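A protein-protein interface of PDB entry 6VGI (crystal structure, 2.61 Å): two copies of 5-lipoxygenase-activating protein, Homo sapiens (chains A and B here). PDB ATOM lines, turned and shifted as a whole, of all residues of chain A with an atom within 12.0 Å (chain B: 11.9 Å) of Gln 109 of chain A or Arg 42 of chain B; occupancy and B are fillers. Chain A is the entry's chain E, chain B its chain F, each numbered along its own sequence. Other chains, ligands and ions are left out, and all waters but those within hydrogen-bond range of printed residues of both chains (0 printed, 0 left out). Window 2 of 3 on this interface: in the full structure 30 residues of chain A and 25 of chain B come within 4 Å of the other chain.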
ATOM      1  N   LEU A  50     -33.197  -1.912   6.323  1.00  0.00           N
ATOM      2  CA  LEU A  50     -31.809  -2.173   5.937  1.00  0.00           C
ATOM      3  C   LEU A  50     -30.799  -1.575   6.916  1.00  0.00           C
ATOM      4  O   LEU A  50     -29.752  -2.167   7.172  1.00  0.00           O
ATOM      5  CB  LEU A  50     -31.549  -1.648   4.520  1.00  0.00           C
ATOM      6  CG  LEU A  50     -30.167  -1.856   3.894  1.00  0.00           C
ATOM      7  CD1 LEU A  50     -29.994  -3.278   3.367  1.00  0.00           C
ATOM      8  CD2 LEU A  50     -29.951  -0.844   2.787  1.00  0.00           C
ATOM      9  N   ALA A  51     -31.122  -0.404   7.459  1.00  0.00           N
ATOM     10  CA  ALA A  51     -30.263   0.267   8.436  1.00  0.00           C
ATOM     11  C   ALA A  51     -30.081  -0.574   9.699  1.00  0.00           C
ATOM     12  O   ALA A  51     -29.001  -0.595  10.284  1.00  0.00           O
ATOM     13  CB  ALA A  51     -30.817   1.638   8.782  1.00  0.00           C
ATOM     14  N   GLU A  53     -30.497  -4.010   9.794  1.00  0.00           N
ATOM     15  CA  GLU A  53     -29.800  -5.238   9.403  1.00  0.00           C
ATOM     16  C   GLU A  53     -28.286  -5.076   9.377  1.00  0.00           C
ATOM     17  O   GLU A  53     -27.557  -5.979   9.793  1.00  0.00           O
ATOM     18  CB  GLU A  53     -30.293  -5.747   8.045  1.00  0.00           C
ATOM     19  CG  GLU A  53     -31.500  -6.675   8.124  1.00  0.00           C
ATOM     20  CD  GLU A  53     -31.149  -8.096   8.556  1.00  0.00           C
ATOM     21  OE1 GLU A  53     -29.952  -8.398   8.766  1.00  0.00           O
ATOM     22  OE2 GLU A  53     -32.082  -8.916   8.680  1.00  0.00           O
ATOM     23  N   ARG A  54     -27.822  -3.925   8.895  1.00  0.00           N
ATOM     24  CA  ARG A  54     -26.391  -3.641   8.787  1.00  0.00           C
ATOM     25  C   ARG A  54     -25.729  -3.448  10.154  1.00  0.00           C
ATOM     26  O   ARG A  54     -24.658  -3.995  10.403  1.00  0.00           O
ATOM     27  CB  ARG A  54     -26.142  -2.426   7.885  1.00  0.00           C
ATOM     28  CG  ARG A  54     -26.490  -2.628   6.409  1.00  0.00           C
ATOM     29  CD  ARG A  54     -25.405  -3.394   5.661  1.00  0.00           C
ATOM     30  NE  ARG A  54     -25.355  -3.030   4.243  1.00  0.00           N
ATOM     31  CZ  ARG A  54     -25.835  -3.771   3.247  1.00  0.00           C
ATOM     32  NH1 ARG A  54     -26.410  -4.943   3.489  1.00  0.00           N
ATOM     33  NH2 ARG A  54     -25.734  -3.337   1.998  1.00  0.00           N
ATOM     34  N   THR A  57     -25.698  -6.866  11.965  1.00  0.00           N
ATOM     35  CA  THR A  57     -24.683  -7.751  11.383  1.00  0.00           C
ATOM     36  C   THR A  57     -23.271  -7.318  11.783  1.00  0.00           C
ATOM     37  O   THR A  57     -22.422  -8.163  12.076  1.00  0.00           O
ATOM     38  CB  THR A  57     -24.804  -7.815   9.843  1.00  0.00           C
ATOM     39  OG1 THR A  57     -26.158  -8.116   9.488  1.00  0.00           O
ATOM     40  CG2 THR A  57     -23.883  -8.883   9.255  1.00  0.00           C
ATOM     41  N   ASN A  61     -20.922  -9.667  14.008  1.00  0.00           N
ATOM     42  CA  ASN A  61     -19.587 -10.027  13.525  1.00  0.00           C
ATOM     43  C   ASN A  61     -18.486  -9.667  14.522  1.00  0.00           C
ATOM     44  O   ASN A  61     -17.532 -10.426  14.696  1.00  0.00           O
ATOM     45  CB  ASN A  61     -19.301  -9.376  12.169  1.00  0.00           C
ATOM     46  CG  ASN A  61     -20.152  -9.950  11.041  1.00  0.00           C
ATOM     47  OD1 ASN A  61     -20.886 -10.924  11.223  1.00  0.00           O
ATOM     48  ND2 ASN A  61     -20.052  -9.341   9.865  1.00  0.00           N
ATOM     49  N   TYR A  99     -14.135  -0.911  11.109  1.00  0.00           N
ATOM     50  CA  TYR A  99     -14.909  -2.041  10.603  1.00  0.00           C
ATOM     51  C   TYR A  99     -16.407  -1.852  10.840  1.00  0.00           C
ATOM     52  O   TYR A  99     -17.212  -2.069   9.935  1.00  0.00           O
ATOM     53  CB  TYR A  99     -14.420  -3.339  11.250  1.00  0.00           C
ATOM     54  CG  TYR A  99     -15.216  -4.574  10.881  1.00  0.00           C
ATOM     55  CD1 TYR A  99     -14.916  -5.298   9.729  1.00  0.00           C
ATOM     56  CD2 TYR A  99     -16.261  -5.024  11.691  1.00  0.00           C
ATOM     57  CE1 TYR A  99     -15.638  -6.431   9.388  1.00  0.00           C
ATOM     58  CE2 TYR A  99     -16.991  -6.154  11.357  1.00  0.00           C
ATOM     59  CZ  TYR A  99     -16.670  -6.856  10.205  1.00  0.00           C
ATOM     60  OH  TYR A  99     -17.387  -7.979   9.866  1.00  0.00           O
ATOM     61  N   VAL A 101     -18.137   1.022  11.600  1.00  0.00           N
ATOM     62  CA  VAL A 101     -18.615   2.196  10.866  1.00  0.00           C
ATOM     63  C   VAL A 101     -18.652   1.914   9.357  1.00  0.00           C
ATOM     64  O   VAL A 101     -19.472   2.483   8.632  1.00  0.00           O
ATOM     65  CB  VAL A 101     -17.757   3.460  11.193  1.00  0.00           C
ATOM     66  CG1 VAL A 101     -18.191   4.673  10.364  1.00  0.00           C
ATOM     67  CG2 VAL A 101     -17.845   3.793  12.680  1.00  0.00           C
ATOM     68  N   GLY A 102     -17.777   1.016   8.903  1.00  0.00           N
ATOM     69  CA  GLY A 102     -17.750   0.568   7.509  1.00  0.00           C
ATOM     70  C   GLY A 102     -19.032  -0.108   7.049  1.00  0.00           C
ATOM     71  O   GLY A 102     -19.280  -0.223   5.846  1.00  0.00           O
ATOM     72  N   TYR A 103     -19.840  -0.562   8.008  1.00  0.00           N
ATOM     73  CA  TYR A 103     -21.154  -1.142   7.732  1.00  0.00           C
ATOM     74  C   TYR A 103     -22.235  -0.069   7.724  1.00  0.00           C
ATOM     75  O   TYR A 103     -23.361  -0.312   7.280  1.00  0.00           O
ATOM     76  CB  TYR A 103     -21.510  -2.188   8.791  1.00  0.00           C
ATOM     77  CG  TYR A 103     -20.973  -3.572   8.521  1.00  0.00           C
ATOM     78  CD1 TYR A 103     -21.797  -4.571   8.011  1.00  0.00           C
ATOM     79  CD2 TYR A 103     -19.644  -3.888   8.793  1.00  0.00           C
ATOM     80  CE1 TYR A 103     -21.307  -5.850   7.765  1.00  0.00           C
ATOM     81  CE2 TYR A 103     -19.143  -5.162   8.550  1.00  0.00           C
ATOM     82  CZ  TYR A 103     -19.979  -6.136   8.038  1.00  0.00           C
ATOM     83  OH  TYR A 103     -19.479  -7.395   7.804  1.00  0.00           O
ATOM     84  N   LEU A 104     -21.884   1.112   8.226  1.00  0.00           N
ATOM     85  CA  LEU A 104     -22.834   2.205   8.402  1.00  0.00           C
ATOM     86  C   LEU A 104     -22.648   3.280   7.335  1.00  0.00           C
ATOM     87  O   LEU A 104     -23.256   3.219   6.266  1.00  0.00           O
ATOM     88  CB  LEU A 104     -22.676   2.811   9.801  1.00  0.00           C
ATOM     89  CG  LEU A 104     -23.387   2.186  11.012  1.00  0.00           C
ATOM     90  CD1 LEU A 104     -23.263   0.665  11.088  1.00  0.00           C
ATOM     91  CD2 LEU A 104     -22.868   2.817  12.295  1.00  0.00           C
ATOM     92  N   THR A 108     -24.915   3.242   0.200  1.00  0.00           N
ATOM     93  CA  THR A 108     -24.068   2.367  -0.609  1.00  0.00           C
ATOM     94  C   THR A 108     -24.368   0.887  -0.362  1.00  0.00           C
ATOM     95  O   THR A 108     -24.979   0.522   0.645  1.00  0.00           O
ATOM     96  CB  THR A 108     -22.552   2.662  -0.404  1.00  0.00           C
ATOM     97  OG1 THR A 108     -21.776   1.879  -1.324  1.00  0.00           O
ATOM     98  CG2 THR A 108     -22.111   2.366   1.036  1.00  0.00           C
ATOM     99  N   GLN A 109     -23.928   0.045  -1.293  1.00  0.00           N
ATOM    100  CA  GLN A 109     -24.222  -1.387  -1.262  1.00  0.00           C
ATOM    101  C   GLN A 109     -23.051  -2.240  -0.756  1.00  0.00           C
ATOM    102  O   GLN A 109     -23.185  -3.456  -0.610  1.00  0.00           O
ATOM    103  CB  GLN A 109     -24.688  -1.861  -2.648  1.00  0.00           C
ATOM    104  CG  GLN A 109     -23.735  -1.526  -3.797  1.00  0.00           C
ATOM    105  CD  GLN A 109     -24.288  -1.891  -5.172  1.00  0.00           C
ATOM    106  OE1 GLN A 109     -25.036  -2.859  -5.327  1.00  0.00           O
ATOM    107  NE2 GLN A 109     -23.903  -1.117  -6.180  1.00  0.00           N
ATOM    108  N   SER A 110     -21.918  -1.596  -0.481  1.00  0.00           N
ATOM    109  CA  SER A 110     -20.687  -2.301  -0.112  1.00  0.00           C
ATOM    110  C   SER A 110     -20.356  -2.184   1.378  1.00  0.00           C
ATOM    111  O   SER A 110     -20.459  -1.103   1.965  1.00  0.00           O
ATOM    112  CB  SER A 110     -19.515  -1.792  -0.957  1.00  0.00           C
ATOM    113  OG  SER A 110     -18.369  -2.605  -0.794  1.00  0.00           O
ATOM    114  N   THR A 111     -19.970  -3.309   1.978  1.00  0.00           N
ATOM    115  CA  THR A 111     -19.508  -3.356   3.370  1.00  0.00           C
ATOM    116  C   THR A 111     -18.234  -4.200   3.458  1.00  0.00           C
ATOM    117  O   THR A 111     -17.886  -4.877   2.492  1.00  0.00           O
ATOM    118  CB  THR A 111     -20.582  -3.948   4.332  1.00  0.00           C
ATOM    119  OG1 THR A 111     -20.765  -5.344   4.064  1.00  0.00           O
ATOM    120  CG2 THR A 111     -21.914  -3.214   4.210  1.00  0.00           C
ATOM    121  N   PRO A 112     -17.527  -4.161   4.609  1.00  0.00           N
ATOM    122  CA  PRO A 112     -16.405  -5.093   4.791  1.00  0.00           C
ATOM    123  C   PRO A 112     -16.877  -6.543   4.962  1.00  0.00           C
ATOM    124  O   PRO A 112     -18.077  -6.793   5.127  1.00  0.00           O
ATOM    125  CB  PRO A 112     -15.734  -4.595   6.080  1.00  0.00           C
ATOM    126  CG  PRO A 112     -16.214  -3.196   6.263  1.00  0.00           C
ATOM    127  CD  PRO A 112     -17.606  -3.188   5.714  1.00  0.00           C
ATOM    128  N   GLY A 113     -15.937  -7.484   4.916  1.00  0.00           N
ATOM    129  CA  GLY A 113     -16.252  -8.906   5.072  1.00  0.00           C
ATOM    130  C   GLY A 113     -16.579  -9.315   6.500  1.00  0.00           C
ATOM    131  O   GLY A 113     -16.946  -8.480   7.331  1.00  0.00           O
ATOM    132  N   TYR A 114     -16.444 -10.607   6.782  1.00  0.00           N
ATOM    133  CA  TYR A 114     -16.757 -11.158   8.101  1.00  0.00           C
ATOM    134  C   TYR A 114     -15.586 -11.038   9.079  1.00  0.00           C
ATOM    135  O   TYR A 114     -15.789 -10.890  10.286  1.00  0.00           O
ATOM    136  CB  TYR A 114     -17.192 -12.622   7.969  1.00  0.00           C
ATOM    137  CG  TYR A 114     -17.541 -13.302   9.274  1.00  0.00           C
ATOM    138  CD1 TYR A 114     -18.679 -12.940   9.994  1.00  0.00           C
ATOM    139  CD2 TYR A 114     -16.737 -14.322   9.784  1.00  0.00           C
ATOM    140  CE1 TYR A 114     -19.002 -13.567  11.194  1.00  0.00           C
ATOM    141  CE2 TYR A 114     -17.053 -14.957  10.981  1.00  0.00           C
ATOM    142  CZ  TYR A 114     -18.184 -14.575  11.680  1.00  0.00           C
ATOM    143  OH  TYR A 114     -18.498 -15.204  12.866  1.00  0.00           O
ATOM    144  N   ILE A 115     -14.370 -11.098   8.543  1.00  0.00           N
ATOM    145  CA  ILE A 115     -13.148 -11.077   9.342  1.00  0.00           C
ATOM    146  C   ILE A 115     -12.511  -9.686   9.351  1.00  0.00           C
ATOM    147  O   ILE A 115     -12.545  -8.967   8.351  1.00  0.00           O
ATOM    148  CB  ILE A 115     -12.126 -12.134   8.832  1.00  0.00           C
ATOM    149  CG1 ILE A 115     -12.756 -13.535   8.826  1.00  0.00           C
ATOM    150  CG2 ILE A 115     -10.851 -12.126   9.680  1.00  0.00           C
ATOM    151  CD1 ILE A 115     -11.975 -14.590   8.039  1.00  0.00           C
ATOM    152  N   GLU B  33     -16.173 -16.761   5.670  1.00  0.00           N
ATOM    153  CA  GLU B  33     -15.746 -15.710   4.749  1.00  0.00           C
ATOM    154  C   GLU B  33     -15.587 -16.226   3.316  1.00  0.00           C
ATOM    155  O   GLU B  33     -15.999 -15.559   2.365  1.00  0.00           O
ATOM    156  CB  GLU B  33     -14.441 -15.071   5.239  1.00  0.00           C
ATOM    157  CG  GLU B  33     -13.993 -13.834   4.463  1.00  0.00           C
ATOM    158  CD  GLU B  33     -14.824 -12.599   4.775  1.00  0.00           C
ATOM    159  OE1 GLU B  33     -16.015 -12.556   4.389  1.00  0.00           O
ATOM    160  OE2 GLU B  33     -14.277 -11.663   5.398  1.00  0.00           O
ATOM    161  N   HIS B  34     -14.990 -17.410   3.181  1.00  0.00           N
ATOM    162  CA  HIS B  34     -14.817 -18.075   1.889  1.00  0.00           C
ATOM    163  C   HIS B  34     -16.170 -18.361   1.241  1.00  0.00           C
ATOM    164  O   HIS B  34     -16.361 -18.118   0.047  1.00  0.00           O
ATOM    165  CB  HIS B  34     -14.027 -19.376   2.070  1.00  0.00           C
ATOM    166  CG  HIS B  34     -13.803 -20.136   0.798  1.00  0.00           C
ATOM    167  ND1 HIS B  34     -14.688 -21.086   0.332  1.00  0.00           N
ATOM    168  CD2 HIS B  34     -12.790 -20.094  -0.099  1.00  0.00           C
ATOM    169  CE1 HIS B  34     -14.231 -21.592  -0.799  1.00  0.00           C
ATOM    170  NE2 HIS B  34     -13.081 -21.008  -1.083  1.00  0.00           N
ATOM    171  N   GLU B  35     -17.100 -18.870   2.042  1.00  0.00           N
ATOM    172  CA  GLU B  35     -18.440 -19.186   1.573  1.00  0.00           C
ATOM    173  C   GLU B  35     -19.249 -17.923   1.281  1.00  0.00           C
ATOM    174  O   GLU B  35     -20.185 -17.947   0.481  1.00  0.00           O
ATOM    175  CB  GLU B  35     -19.162 -20.069   2.595  1.00  0.00           C
ATOM    176  CG  GLU B  35     -20.267 -20.934   2.011  1.00  0.00           C
ATOM    177  CD  GLU B  35     -19.806 -21.790   0.846  1.00  0.00           C
ATOM    178  OE1 GLU B  35     -18.788 -22.503   0.984  1.00  0.00           O
ATOM    179  OE2 GLU B  35     -20.472 -21.748  -0.209  1.00  0.00           O
ATOM    180  N   SER B  36     -18.880 -16.822   1.931  1.00  0.00           N
ATOM    181  CA  SER B  36     -19.516 -15.533   1.681  1.00  0.00           C
ATOM    182  C   SER B  36     -19.116 -14.963   0.320  1.00  0.00           C
ATOM    183  O   SER B  36     -19.944 -14.371  -0.376  1.00  0.00           O
ATOM    184  CB  SER B  36     -19.183 -14.538   2.792  1.00  0.00           C
ATOM    185  OG  SER B  36     -19.879 -13.322   2.598  1.00  0.00           O
ATOM    186  N   ARG B  37     -17.854 -15.150  -0.059  1.00  0.00           N
ATOM    187  CA  ARG B  37     -17.369 -14.659  -1.352  1.00  0.00           C
ATOM    188  C   ARG B  37     -17.672 -15.587  -2.540  1.00  0.00           C
ATOM    189  O   ARG B  37     -17.331 -15.259  -3.679  1.00  0.00           O
ATOM    190  CB  ARG B  37     -15.885 -14.254  -1.297  1.00  0.00           C
ATOM    191  CG  ARG B  37     -14.921 -15.315  -0.786  1.00  0.00           C
ATOM    192  CD  ARG B  37     -13.516 -14.749  -0.578  1.00  0.00           C
ATOM    193  NE  ARG B  37     -13.501 -13.587   0.314  1.00  0.00           N
ATOM    194  CZ  ARG B  37     -12.400 -13.007   0.789  1.00  0.00           C
ATOM    195  NH1 ARG B  37     -11.198 -13.475   0.472  1.00  0.00           N
ATOM    196  NH2 ARG B  37     -12.501 -11.955   1.590  1.00  0.00           N
ATOM    197  N   THR B  38     -18.318 -16.727  -2.280  1.00  0.00           N
ATOM    198  CA  THR B  38     -18.886 -17.546  -3.359  1.00  0.00           C
ATOM    199  C   THR B  38     -20.085 -16.814  -3.951  1.00  0.00           C
ATOM    200  O   THR B  38     -20.366 -16.926  -5.145  1.00  0.00           O
ATOM    201  CB  THR B  38     -19.316 -18.960  -2.900  1.00  0.00           C
ATOM    202  OG1 THR B  38     -20.361 -18.860  -1.923  1.00  0.00           O
ATOM    203  CG2 THR B  38     -18.135 -19.738  -2.328  1.00  0.00           C
ATOM    204  N   GLN B  39     -20.796 -16.079  -3.096  1.00  0.00           N
ATOM    205  CA  GLN B  39     -21.739 -15.062  -3.539  1.00  0.00           C
ATOM    206  C   GLN B  39     -20.935 -13.838  -3.957  1.00  0.00           C
ATOM    207  O   GLN B  39     -19.874 -13.566  -3.392  1.00  0.00           O
ATOM    208  CB  GLN B  39     -22.715 -14.682  -2.424  1.00  0.00           C
ATOM    209  CG  GLN B  39     -23.810 -15.708  -2.160  1.00  0.00           C
ATOM    210  CD  GLN B  39     -23.439 -16.700  -1.077  1.00  0.00           C
ATOM    211  OE1 GLN B  39     -23.263 -16.330   0.084  1.00  0.00           O
ATOM    212  NE2 GLN B  39     -23.331 -17.970  -1.448  1.00  0.00           N
ATOM    213  N   ASN B  40     -21.435 -13.104  -4.945  1.00  0.00           N
ATOM    214  CA  ASN B  40     -20.739 -11.923  -5.443  1.00  0.00           C
ATOM    215  C   ASN B  40     -21.521 -10.642  -5.182  1.00  0.00           C
ATOM    216  O   ASN B  40     -21.868 -10.345  -4.038  1.00  0.00           O
ATOM    217  CB  ASN B  40     -20.420 -12.074  -6.933  1.00  0.00           C
ATOM    218  CG  ASN B  40     -19.457 -13.219  -7.213  1.00  0.00           C
ATOM    219  OD1 ASN B  40     -18.331 -13.237  -6.718  1.00  0.00           O
ATOM    220  ND2 ASN B  40     -19.898 -14.178  -8.020  1.00  0.00           N
ATOM    221  N   ARG B  42     -21.069  -8.176  -2.607  1.00  0.00           N
ATOM    222  CA  ARG B  42     -20.504  -6.839  -2.464  1.00  0.00           C
ATOM    223  C   ARG B  42     -20.466  -6.430  -0.989  1.00  0.00           C
ATOM    224  O   ARG B  42     -19.498  -5.818  -0.529  1.00  0.00           O
ATOM    225  CB  ARG B  42     -21.310  -5.832  -3.289  1.00  0.00           C
ATOM    226  CG  ARG B  42     -20.460  -4.838  -4.068  1.00  0.00           C
ATOM    227  CD  ARG B  42     -21.273  -4.175  -5.172  1.00  0.00           C
ATOM    228  NE  ARG B  42     -20.429  -3.522  -6.173  1.00  0.00           N
ATOM    229  CZ  ARG B  42     -20.111  -2.229  -6.175  1.00  0.00           C
ATOM    230  NH1 ARG B  42     -20.563  -1.418  -5.224  1.00  0.00           N
ATOM    231  NH2 ARG B  42     -19.336  -1.741  -7.134  1.00  0.00           N
ATOM    232  N   SER B  43     -21.528  -6.773  -0.262  1.00  0.00           N
ATOM    233  CA  SER B  43     -21.593  -6.592   1.184  1.00  0.00           C
ATOM    234  C   SER B  43     -21.674  -7.948   1.881  1.00  0.00           C
ATOM    235  O   SER B  43     -21.939  -8.966   1.236  1.00  0.00           O
ATOM    236  CB  SER B  43     -22.808  -5.741   1.563  1.00  0.00           C
ATOM    237  OG  SER B  43     -24.020  -6.376   1.196  1.00  0.00           O
ATOM    238  N   PHE B  44     -21.440  -7.965   3.192  1.00  0.00           N
ATOM    239  CA  PHE B  44     -21.627  -9.186   3.968  1.00  0.00           C
ATOM    240  C   PHE B  44     -23.042  -9.266   4.523  1.00  0.00           C
ATOM    241  O   PHE B  44     -23.531  -8.324   5.152  1.00  0.00           O
ATOM    242  CB  PHE B  44     -20.601  -9.320   5.098  1.00  0.00           C
ATOM    243  CG  PHE B  44     -20.682 -10.635   5.830  1.00  0.00           C
ATOM    244  CD1 PHE B  44     -21.476 -10.770   6.969  1.00  0.00           C
ATOM    245  CD2 PHE B  44     -19.981 -11.747   5.367  1.00  0.00           C
ATOM    246  CE1 PHE B  44     -21.565 -11.986   7.639  1.00  0.00           C
ATOM    247  CE2 PHE B  44     -20.064 -12.967   6.029  1.00  0.00           C
ATOM    248  CZ  PHE B  44     -20.856 -13.087   7.169  1.00  0.00           C
ATOM    249  N   GLN B  45     -23.685 -10.406   4.279  1.00  0.00           N
ATOM    250  CA  GLN B  45     -25.035 -10.680   4.757  1.00  0.00           C
ATOM    251  C   GLN B  45     -25.029 -11.975   5.559  1.00  0.00           C
ATOM    252  O   GLN B  45     -24.172 -12.832   5.346  1.00  0.00           O
ATOM    253  CB  GLN B  45     -26.002 -10.811   3.577  1.00  0.00           C
ATOM    254  CG  GLN B  45     -26.095  -9.584   2.676  1.00  0.00           C
ATOM    255  CD  GLN B  45     -27.338  -9.600   1.805  1.00  0.00           C
ATOM    256  OE1 GLN B  45     -27.267  -9.863   0.604  1.00  0.00           O
ATOM    257  NE2 GLN B  45     -28.491  -9.330   2.414  1.00  0.00           N
ATOM    258  N   ARG B  46     -25.982 -12.115   6.479  1.00  0.00           N
ATOM    259  CA  ARG B  46     -26.102 -13.334   7.289  1.00  0.00           C
ATOM    260  C   ARG B  46     -27.046 -14.379   6.679  1.00  0.00           C
ATOM    261  O   ARG B  46     -27.195 -15.479   7.215  1.00  0.00           O
ATOM    262  CB  ARG B  46     -26.457 -13.021   8.752  1.00  0.00           C
ATOM    263  CG  ARG B  46     -27.272 -11.756   8.969  1.00  0.00           C
ATOM    264  CD  ARG B  46     -27.125 -11.246  10.398  1.00  0.00           C
ATOM    265  NE  ARG B  46     -27.898 -12.039  11.354  1.00  0.00           N
ATOM    266  CZ  ARG B  46     -29.160 -11.790  11.696  1.00  0.00           C
ATOM    267  NH1 ARG B  46     -29.815 -10.762  11.167  1.00  0.00           N
ATOM    268  NH2 ARG B  46     -29.771 -12.572  12.574  1.00  0.00           N
ATOM    269  N   THR B  47     -27.679 -14.024   5.563  1.00  0.00           N
ATOM    270  CA  THR B  47     -28.466 -14.972   4.770  1.00  0.00           C
ATOM    271  C   THR B  47     -27.806 -15.154   3.402  1.00  0.00           C
ATOM    272  O   THR B  47     -26.994 -14.324   2.985  1.00  0.00           O
ATOM    273  CB  THR B  47     -29.943 -14.520   4.585  1.00  0.00           C
ATOM    274  OG1 THR B  47     -30.003 -13.392   3.702  1.00  0.00           O
ATOM    275  CG2 THR B  47     -30.588 -14.159   5.924  1.00  0.00           C
ATOM    276  N   GLY B  48     -28.152 -16.239   2.714  1.00  0.00           N
ATOM    277  CA  GLY B  48     -27.606 -16.521   1.389  1.00  0.00           C
ATOM    278  C   GLY B  48     -27.965 -17.902   0.877  1.00  0.00           C
ATOM    279  O   GLY B  48     -29.035 -18.431   1.185  1.00  0.00           O
ATOM    280  N   PHE B  52     -23.859 -21.394   2.322  1.00  0.00           N
ATOM    281  CA  PHE B  52     -23.442 -20.317   3.218  1.00  0.00           C
ATOM    282  C   PHE B  52     -24.178 -20.359   4.553  1.00  0.00           C
ATOM    283  O   PHE B  52     -23.560 -20.232   5.610  1.00  0.00           O
ATOM    284  CB  PHE B  52     -23.607 -18.939   2.557  1.00  0.00           C
ATOM    285  CG  PHE B  52     -23.362 -17.786   3.496  1.00  0.00           C
ATOM    286  CD1 PHE B  52     -22.070 -17.474   3.914  1.00  0.00           C
ATOM    287  CD2 PHE B  52     -24.423 -17.024   3.974  1.00  0.00           C
ATOM    288  CE1 PHE B  52     -21.837 -16.417   4.791  1.00  0.00           C
ATOM    289  CE2 PHE B  52     -24.201 -15.964   4.853  1.00  0.00           C
ATOM    290  CZ  PHE B  52     -22.902 -15.661   5.261  1.00  0.00           C
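N of Tyr 114 of chain A is in hydrogen-bond range of OE2 of Glu 33 of chain B, at 2.8 Å. OE1 of Glu 53 of chain A is in salt-bridge range of NH1 of Arg 46 of chain B (3.4 Å). The guanidinium group of Arg 42 of chain B lies close to the side-chain amide nitrogen of Gln 109 of chain A, 3.5 Å away. The backbone NH of Ile 115 of chain A is in hydrogen-bond range of the side-chain carboxylate of Glu 33 of chain B, 3.2 Å away. The side-chain hydroxyl (OG) of Ser 110 of chain A lies within hydrogen-bond range of the backbone carbonyl oxygen (O) of Arg 42 of chain B, 3.4 Å away. N of Phe 44 of chain B is in hydrogen-bond range of OG1 of Thr 111 of chain A (2.8 Å).
The side-chain hydroxyl (OH) of Tyr 103 of chain A sits at hydrogen-bond distance from the backbone carbonyl oxygen (O) of Gly 113 of chain A, 2.8 Å away. The side-chain hydroxyl of Tyr 99 of chain A is in hydrogen-bond range of the backbone carbonyl oxygen of Tyr 114 of chain A (3.3 Å). The side-chain amide nitrogen (ND2) of Asn 61 of chain A lies within hydrogen-bond range of the side-chain hydroxyl (OH) of Tyr 99 of chain A (3.0 Å). ND2 of Asn 61 of chain A is in hydrogen-bond range of OH of Tyr 103 of chain A (2.9 Å). O of Pro 112 of chain A lies within hydrogen-bond range of OH of Tyr 103 of chain A, 3.1 Å away. The backbone carbonyl oxygen (O) of Thr 57 of chain A lies close to the side-chain amide oxygen (OD1) of Asn 61 of chain A, at 3.3 Å.
Of the 19 printed residues of chain A, 12 touch a printed residue of chain B. Hydrophobic or aromatic side chains of chain A that line the printed part of chain B: Tyr 103, Tyr 114 and Ile 115. Among the printed residues, Asp or Glu carboxylates within 4 Å of a Lys or Arg side-chain nitrogen of the other chain: Glu 53 of chain A with Arg 46 of chain B.
Printed residues of chain B within 4 Å of Asn 61 of chain A: Phe 44 (3.5 Å). Of the printed residues of chain B, Tyr 103 of chain A touches Phe 44. No residue of chain B comes within 4 Å of Thr 108 of chain A. Gln 109 of chain A touches two residues of chain B. Of the printed residues of chain B, Pro 112 of chain A touches Phe 44 (3.6 Å). Printed residues of chain B within 4 Å of Gly 113 of chain A: Glu 33 (3.4 Å). Printed residues of chain B within 4 Å of Tyr 114 of chain A: Glu 33 (2.8 Å) and Phe 44 (3.5 Å). Glu 35 of chain B touches none of the printed residues of chain A. Thr 38 of chain B touches none of the printed residues of chain A. Arg 42 of chain B touches three residues of chain A. Ser 43 of chain B touches just these residues of chain A: Arg 54, Gln 109 and Thr 111.
Among the printed residues, merely in contact across the chains: Gln 109 of chain A with Ser 43 of chain B (3.2 Å), Thr 111 of chain A with Ser 43 of chain B (3.2 Å), Thr 57 of chain A with Arg 46 of chain B (3.4 Å), Gly 113 of chain A with Glu 33 of chain B (3.4 Å), Tyr 114 of chain A with Phe 44 of chain B (3.5 Å), Tyr 103 of chain A with Phe 44 of chain B (3.5 Å), Asn 61 of chain A with Phe 44 of chain B (3.5 Å), Thr 111 of chain A with Arg 42 of chain B (3.6 Å), Pro 112 of chain A with Phe 44 of chain B (3.6 Å), Arg 54 of chain A with Ser 43 of chain B (3.6 Å) and Thr 57 of chain A with Phe 44 of chain B (3.8 Å).
No position is printed for both chains.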
